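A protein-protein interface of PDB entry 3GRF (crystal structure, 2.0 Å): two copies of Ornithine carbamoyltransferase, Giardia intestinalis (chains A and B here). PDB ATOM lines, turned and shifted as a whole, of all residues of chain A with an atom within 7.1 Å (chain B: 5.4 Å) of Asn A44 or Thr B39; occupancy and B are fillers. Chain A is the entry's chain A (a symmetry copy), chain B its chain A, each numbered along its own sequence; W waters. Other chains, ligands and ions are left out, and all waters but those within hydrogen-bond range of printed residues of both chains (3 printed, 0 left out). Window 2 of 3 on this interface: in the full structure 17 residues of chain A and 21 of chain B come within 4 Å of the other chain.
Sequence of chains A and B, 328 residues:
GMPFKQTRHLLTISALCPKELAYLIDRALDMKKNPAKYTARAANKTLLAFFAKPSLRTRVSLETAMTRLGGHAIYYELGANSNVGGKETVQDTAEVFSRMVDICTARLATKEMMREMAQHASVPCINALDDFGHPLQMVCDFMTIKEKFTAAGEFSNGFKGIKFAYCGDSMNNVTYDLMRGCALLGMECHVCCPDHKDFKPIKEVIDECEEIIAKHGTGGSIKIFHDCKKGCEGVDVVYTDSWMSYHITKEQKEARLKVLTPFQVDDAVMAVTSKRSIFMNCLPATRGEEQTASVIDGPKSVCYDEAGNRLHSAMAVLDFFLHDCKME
Asn A44 touches just these residues of chain B: Thr B39 (3.0 Å), Thr B67 (2.9 Å), Arg B68 (3.5 Å) and Gly B70 (3.8 Å). Of the printed residues of chain B, Lys A45 touches Thr B67. Of the printed residues of chain B, Thr A46 touches Thr B67 (3.7 Å). Of the printed residues of chain B, His A72 touches Thr B67 (3.4 Å). Thr B39 touches one residue of chain A. Of the printed residues of chain A, Thr B67 touches Asn A44 (2.9 Å), Lys A45 (3.7 Å), Thr A46 (3.7 Å) and His A72 (3.4 Å). Of the printed residues of chain A, Gly B70 touches Asn A44. The nearest printed residue of chain B that does not touch Thr A46 is Arg B68 (5.3 Å).
Gly B70 touches Asn A44 (CA to OD1, 3.8 Å). CG2 of Thr B67 touches O of Lys A45 (3.7 Å). CG2 of Thr A46 touches CB of Thr B67, 3.7 Å away. Thr B67 touches His A72 (OG1 to CB, 3.4 Å).
Printed residues of chain B that touch a printed residue of chain A: Thr B39, Thr B67, Arg B68 and Gly B70. Hydrophobic or aromatic side chains of chain A that line the printed part of chain B: His A72. Among the printed residues, no Asp or Glu carboxylate lies within 4 Å of a Lys or Arg side-chain nitrogen of the other chain.
Water W3 bridges OD2 of Asp A102 (2.6 Å) and NH1 of Arg B68 (3.4 Å). Water W2 lies within hydrogen-bond range of OG1 of Thr B67 (2.6 Å) and ND1 of His A72 (2.8 Å). Water W1 lies within hydrogen-bond range of the guanidinium group (NH1) of Arg B68 and the side-chain carboxylate (OD1) of Asp A102.
Positions printed for both chains: 40, 41, 69 and 70.
The backbone carbonyl oxygen (O) of Lys A45 is in hydrogen-bond range of the backbone NH (N) of His A72, 3.2 Å away. N of Thr A46 is in hydrogen-bond range of OD1 of Asp A102.
ND2 of Asn A44 sits at hydrogen-bond distance from OG1 of Thr B39 (3.0 Å). The backbone carbonyl oxygen of Thr B67 lies close to the side-chain amide oxygen of Asn A44. O of Arg B68 sits close to OD1 of Asn A44 (3.5 Å).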
ATOM      1  N   ALA A  40      16.555 -31.250  23.644  1.00  0.00           N
ATOM      2  CA  ALA A  40      15.717 -30.058  23.766  1.00  0.00           C
ATOM      3  C   ALA A  40      16.572 -28.789  23.782  1.00  0.00           C
ATOM      4  O   ALA A  40      16.090 -27.696  24.096  1.00  0.00           O
ATOM      5  CB  ALA A  40      14.858 -30.153  24.999  1.00  0.00           C
ATOM      6  N   ARG A  41      17.844 -28.937  23.419  1.00  0.00           N
ATOM      7  CA  ARG A  41      18.800 -27.815  23.392  1.00  0.00           C
ATOM      8  C   ARG A  41      18.411 -26.679  22.430  1.00  0.00           C
ATOM      9  O   ARG A  41      18.567 -25.497  22.773  1.00  0.00           O
ATOM     10  CB  ARG A  41      20.217 -28.328  23.097  1.00  0.00           C
ATOM     11  CG  ARG A  41      20.898 -29.130  24.245  1.00  0.00           C
ATOM     12  CD  ARG A  41      21.131 -28.289  25.531  1.00  0.00           C
ATOM     13  NE  ARG A  41      22.171 -27.284  25.303  1.00  0.00           N
ATOM     14  CZ  ARG A  41      22.691 -26.457  26.211  1.00  0.00           C
ATOM     15  NH1 ARG A  41      22.285 -26.449  27.468  1.00  0.00           N
ATOM     16  NH2 ARG A  41      23.655 -25.633  25.836  1.00  0.00           N
ATOM     17  N   ALA A  42      17.852 -27.022  21.265  1.00  0.00           N
ATOM     18  CA  ALA A  42      17.334 -26.009  20.312  1.00  0.00           C
ATOM     19  C   ALA A  42      15.824 -26.054  20.142  1.00  0.00           C
ATOM     20  O   ALA A  42      15.315 -25.665  19.100  1.00  0.00           O
ATOM     21  CB  ALA A  42      18.015 -26.191  18.892  1.00  0.00           C
ATOM     22  N   ALA A  43      15.094 -26.531  21.140  1.00  0.00           N
ATOM     23  CA  ALA A  43      13.657 -26.606  21.032  1.00  0.00           C
ATOM     24  C   ALA A  43      13.143 -25.237  20.604  1.00  0.00           C
ATOM     25  O   ALA A  43      13.567 -24.231  21.164  1.00  0.00           O
ATOM     26  CB  ALA A  43      13.044 -27.000  22.396  1.00  0.00           C
ATOM     27  N   ASN A  44      12.232 -25.210  19.608  1.00  0.00           N
ATOM     28  CA  ASN A  44      11.597 -23.981  19.077  1.00  0.00           C
ATOM     29  C   ASN A  44      12.495 -22.961  18.410  1.00  0.00           C
ATOM     30  O   ASN A  44      12.084 -21.800  18.127  1.00  0.00           O
ATOM     31  CB  ASN A  44      10.732 -23.289  20.117  1.00  0.00           C
ATOM     32  CG  ASN A  44       9.673 -24.202  20.667  1.00  0.00           C
ATOM     33  OD1 ASN A  44       8.670 -24.467  20.017  1.00  0.00           O
ATOM     34  ND2 ASN A  44       9.929 -24.748  21.839  1.00  0.00           N
ATOM     35  N   LYS A  45      13.740 -23.361  18.193  1.00  0.00           N
ATOM     36  CA  LYS A  45      14.726 -22.411  17.678  1.00  0.00           C
ATOM     37  C   LYS A  45      14.984 -22.830  16.274  1.00  0.00           C
ATOM     38  O   LYS A  45      14.854 -24.025  15.979  1.00  0.00           O
ATOM     39  CB  LYS A  45      16.010 -22.427  18.514  1.00  0.00           C
ATOM     40  CG  LYS A  45      15.825 -21.692  19.865  1.00  0.00           C
ATOM     41  CD  LYS A  45      16.982 -21.977  20.810  1.00  0.00           C
ATOM     42  CE  LYS A  45      16.755 -21.314  22.174  1.00  0.00           C
ATOM     43  NZ  LYS A  45      17.236 -19.904  22.159  1.00  0.00           N
ATOM     44  N   THR A  46      15.295 -21.904  15.353  1.00  0.00           N
ATOM     45  CA  THR A  46      15.524 -22.296  13.940  1.00  0.00           C
ATOM     46  C   THR A  46      16.836 -21.794  13.397  1.00  0.00           C
ATOM     47  O   THR A  46      17.340 -20.740  13.789  1.00  0.00           O
ATOM     48  CB  THR A  46      14.359 -21.881  12.977  1.00  0.00           C
ATOM     49  OG1 THR A  46      14.805 -20.799  12.139  1.00  0.00           O
ATOM     50  CG2 THR A  46      13.150 -21.460  13.791  1.00  0.00           C
ATOM     51  N   MET A  66      19.688 -30.164  13.714  1.00  0.00           N
ATOM     52  CA  MET A  66      18.676 -29.345  14.395  1.00  0.00           C
ATOM     53  C   MET A  66      17.560 -30.174  14.922  1.00  0.00           C
ATOM     54  O   MET A  66      17.102 -29.935  16.028  1.00  0.00           O
ATOM     55  CB  MET A  66      18.126 -28.216  13.513  1.00  0.00           C
ATOM     56  CG  MET A  66      19.143 -27.122  13.141  1.00  0.00           C
ATOM     57  SD  MET A  66      19.734 -26.119  14.536  1.00  0.00           S
ATOM     58  CE  MET A  66      18.196 -25.377  15.014  1.00  0.00           C
ATOM     59  N   LEU A  69      18.453 -31.799  18.205  1.00  0.00           N
ATOM     60  CA  LEU A  69      18.568 -30.788  19.244  1.00  0.00           C
ATOM     61  C   LEU A  69      17.178 -30.280  19.526  1.00  0.00           C
ATOM     62  O   LEU A  69      16.976 -29.614  20.517  1.00  0.00           O
ATOM     63  CB  LEU A  69      19.442 -29.646  18.737  1.00  0.00           C
ATOM     64  CG  LEU A  69      20.909 -29.419  19.098  1.00  0.00           C
ATOM     65  CD1 LEU A  69      21.568 -30.497  19.899  1.00  0.00           C
ATOM     66  CD2 LEU A  69      21.693 -29.120  17.831  1.00  0.00           C
ATOM     67  N   GLY A  70      16.232 -30.571  18.623  1.00  0.00           N
ATOM     68  CA  GLY A  70      14.794 -30.345  18.838  1.00  0.00           C
ATOM     69  C   GLY A  70      14.247 -29.096  18.193  1.00  0.00           C
ATOM     70  O   GLY A  70      13.157 -28.624  18.548  1.00  0.00           O
ATOM     71  N   GLY A  71      15.010 -28.561  17.247  1.00  0.00           N
ATOM     72  CA  GLY A  71      14.692 -27.297  16.612  1.00  0.00           C
ATOM     73  C   GLY A  71      14.505 -27.636  15.144  1.00  0.00           C
ATOM     74  O   GLY A  71      14.116 -28.769  14.816  1.00  0.00           O
ATOM     75  N   HIS A  72      14.784 -26.676  14.274  1.00  0.00           N
ATOM     76  CA  HIS A  72      14.452 -26.831  12.830  1.00  0.00           C
ATOM     77  C   HIS A  72      15.402 -26.010  11.991  1.00  0.00           C
ATOM     78  O   HIS A  72      15.779 -24.929  12.403  1.00  0.00           O
ATOM     79  CB  HIS A  72      13.034 -26.338  12.538  1.00  0.00           C
ATOM     80  CG  HIS A  72      12.586 -26.646  11.143  1.00  0.00           C
ATOM     81  ND1 HIS A  72      12.349 -25.668  10.203  1.00  0.00           N
ATOM     82  CD2 HIS A  72      12.407 -27.828  10.511  1.00  0.00           C
ATOM     83  CE1 HIS A  72      12.024 -26.230   9.053  1.00  0.00           C
ATOM     84  NE2 HIS A  72      12.043 -27.541   9.211  1.00  0.00           N
ATOM     85  N   ASP A 102      17.446 -17.748  14.868  1.00  0.00           N
ATOM     86  CA  ASP A 102      18.381 -17.774  15.983  1.00  0.00           C
ATOM     87  C   ASP A 102      19.820 -17.950  15.513  1.00  0.00           C
ATOM     88  O   ASP A 102      20.792 -17.612  16.210  1.00  0.00           O
ATOM     89  CB  ASP A 102      17.983 -18.891  16.930  1.00  0.00           C
ATOM     90  CG  ASP A 102      16.610 -18.721  17.439  1.00  0.00           C
ATOM     91  OD1 ASP A 102      15.686 -19.377  16.913  1.00  0.00           O
ATOM     92  OD2 ASP A 102      16.429 -17.866  18.314  1.00  0.00           O
ATOM     93  N   PRO B  35       7.328 -15.553  24.295  1.00  0.00           N
ATOM     94  CA  PRO B  35       7.226 -16.687  23.405  1.00  0.00           C
ATOM     95  C   PRO B  35       7.146 -18.031  24.164  1.00  0.00           C
ATOM     96  O   PRO B  35       6.555 -19.000  23.686  1.00  0.00           O
ATOM     97  CB  PRO B  35       8.499 -16.563  22.575  1.00  0.00           C
ATOM     98  CG  PRO B  35       9.442 -15.774  23.407  1.00  0.00           C
ATOM     99  CD  PRO B  35       8.601 -14.833  24.127  1.00  0.00           C
ATOM    100  N   ALA B  36       7.696 -18.090  25.373  1.00  0.00           N
ATOM    101  CA  ALA B  36       7.714 -19.321  26.084  1.00  0.00           C
ATOM    102  C   ALA B  36       6.317 -19.880  26.300  1.00  0.00           C
ATOM    103  O   ALA B  36       6.162 -21.068  26.555  1.00  0.00           O
ATOM    104  CB  ALA B  36       8.423 -19.115  27.427  1.00  0.00           C
ATOM    105  N   LYS B  37       5.291 -19.038  26.263  1.00  0.00           N
ATOM    106  CA  LYS B  37       3.917 -19.488  26.521  1.00  0.00           C
ATOM    107  C   LYS B  37       3.304 -20.278  25.348  1.00  0.00           C
ATOM    108  O   LYS B  37       2.366 -21.052  25.519  1.00  0.00           O
ATOM    109  CB  LYS B  37       3.031 -18.276  26.786  1.00  0.00           C
ATOM    110  CG  LYS B  37       3.092 -17.753  28.204  1.00  0.00           C
ATOM    111  CD  LYS B  37       2.501 -16.335  28.311  1.00  0.00           C
ATOM    112  CE  LYS B  37       1.095 -16.242  27.705  1.00  0.00           C
ATOM    113  NZ  LYS B  37       0.070 -17.206  28.284  1.00  0.00           N
ATOM    114  N   TYR B  38       3.808 -20.032  24.146  1.00  0.00           N
ATOM    115  CA  TYR B  38       3.164 -20.467  22.911  1.00  0.00           C
ATOM    116  C   TYR B  38       3.871 -21.647  22.248  1.00  0.00           C
ATOM    117  O   TYR B  38       3.614 -22.029  21.098  1.00  0.00           O
ATOM    118  CB  TYR B  38       3.152 -19.282  21.964  1.00  0.00           C
ATOM    119  CG  TYR B  38       2.335 -18.166  22.520  1.00  0.00           C
ATOM    120  CD1 TYR B  38       2.921 -17.128  23.270  1.00  0.00           C
ATOM    121  CD2 TYR B  38       0.965 -18.174  22.337  1.00  0.00           C
ATOM    122  CE1 TYR B  38       2.138 -16.118  23.780  1.00  0.00           C
ATOM    123  CE2 TYR B  38       0.189 -17.185  22.837  1.00  0.00           C
ATOM    124  CZ  TYR B  38       0.764 -16.151  23.542  1.00  0.00           C
ATOM    125  OH  TYR B  38      -0.095 -15.171  23.992  1.00  0.00           O
ATOM    126  N   THR B  39       4.725 -22.258  23.024  1.00  0.00           N
ATOM    127  CA  THR B  39       5.722 -23.144  22.530  1.00  0.00           C
ATOM    128  C   THR B  39       5.182 -24.526  22.071  1.00  0.00           C
ATOM    129  O   THR B  39       5.891 -25.320  21.435  1.00  0.00           O
ATOM    130  CB  THR B  39       6.791 -23.143  23.606  1.00  0.00           C
ATOM    131  OG1 THR B  39       8.035 -22.762  23.022  1.00  0.00           O
ATOM    132  CG2 THR B  39       6.873 -24.391  24.318  1.00  0.00           C
ATOM    133  N   ALA B  40       3.919 -24.809  22.373  1.00  0.00           N
ATOM    134  CA  ALA B  40       3.309 -26.098  22.050  1.00  0.00           C
ATOM    135  C   ALA B  40       1.935 -25.905  21.405  1.00  0.00           C
ATOM    136  O   ALA B  40       1.159 -26.855  21.255  1.00  0.00           O
ATOM    137  CB  ALA B  40       3.216 -26.951  23.287  1.00  0.00           C
ATOM    138  N   ARG B  41       1.648 -24.670  21.001  1.00  0.00           N
ATOM    139  CA  ARG B  41       0.362 -24.317  20.370  1.00  0.00           C
ATOM    140  C   ARG B  41       0.079 -25.066  19.057  1.00  0.00           C
ATOM    141  O   ARG B  41      -1.062 -25.490  18.820  1.00  0.00           O
ATOM    142  CB  ARG B  41       0.264 -22.797  20.173  1.00  0.00           C
ATOM    143  CG  ARG B  41       0.076 -21.958  21.471  1.00  0.00           C
ATOM    144  CD  ARG B  41      -1.255 -22.264  22.215  1.00  0.00           C
ATOM    145  NE  ARG B  41      -2.396 -21.762  21.448  1.00  0.00           N
ATOM    146  CZ  ARG B  41      -3.675 -21.765  21.829  1.00  0.00           C
ATOM    147  NH1 ARG B  41      -4.060 -22.265  22.990  1.00  0.00           N
ATOM    148  NH2 ARG B  41      -4.576 -21.236  21.021  1.00  0.00           N
ATOM    149  N   THR B  67       7.824 -23.343  13.828  1.00  0.00           N
ATOM    150  CA  THR B  67       8.802 -23.902  14.797  1.00  0.00           C
ATOM    151  C   THR B  67       8.589 -23.318  16.180  1.00  0.00           C
ATOM    152  O   THR B  67       8.680 -24.020  17.201  1.00  0.00           O
ATOM    153  CB  THR B  67      10.234 -23.628  14.328  1.00  0.00           C
ATOM    154  OG1 THR B  67      10.389 -24.190  13.015  1.00  0.00           O
ATOM    155  CG2 THR B  67      11.277 -24.255  15.275  1.00  0.00           C
ATOM    156  N   ARG B  68       8.293 -22.029  16.238  1.00  0.00           N
ATOM    157  CA  ARG B  68       8.129 -21.357  17.551  1.00  0.00           C
ATOM    158  C   ARG B  68       6.893 -21.773  18.320  1.00  0.00           C
ATOM    159  O   ARG B  68       6.814 -21.591  19.535  1.00  0.00           O
ATOM    160  CB  ARG B  68       8.189 -19.851  17.385  1.00  0.00           C
ATOM    161  CG  ARG B  68       9.629 -19.390  17.158  1.00  0.00           C
ATOM    162  CD  ARG B  68       9.691 -17.931  16.791  1.00  0.00           C
ATOM    163  NE  ARG B  68       9.553 -17.026  17.939  1.00  0.00           N
ATOM    164  CZ  ARG B  68      10.561 -16.437  18.582  1.00  0.00           C
ATOM    165  NH1 ARG B  68      11.808 -16.680  18.227  1.00  0.00           N
ATOM    166  NH2 ARG B  68      10.315 -15.611  19.610  1.00  0.00           N
ATOM    167  N   LEU B  69       5.923 -22.295  17.563  1.00  0.00           N
ATOM    168  CA  LEU B  69       4.624 -22.754  18.026  1.00  0.00           C
ATOM    169  C   LEU B  69       4.719 -24.246  18.211  1.00  0.00           C
ATOM    170  O   LEU B  69       3.851 -24.828  18.821  1.00  0.00           O
ATOM    171  CB  LEU B  69       3.572 -22.432  16.969  1.00  0.00           C
ATOM    172  CG  LEU B  69       2.585 -21.268  17.021  1.00  0.00           C
ATOM    173  CD1 LEU B  69       2.775 -20.288  18.135  1.00  0.00           C
ATOM    174  CD2 LEU B  69       2.568 -20.568  15.672  1.00  0.00           C
ATOM    175  N   GLY B  70       5.767 -24.860  17.646  1.00  0.00           N
ATOM    176  CA  GLY B  70       6.134 -26.262  17.902  1.00  0.00           C
ATOM    177  C   GLY B  70       5.691 -27.236  16.838  1.00  0.00           C
ATOM    178  O   GLY B  70       5.649 -28.453  17.070  1.00  0.00           O
HETATM  179  O   HOH W   1      13.280 -17.869  16.107  1.00  0.00           O
HETATM  180  O   HOH W   2      11.823 -23.089  11.191  1.00  0.00           O
HETATM  181  O   HOH W   3      14.497 -17.874  20.004  1.00  0.00           O
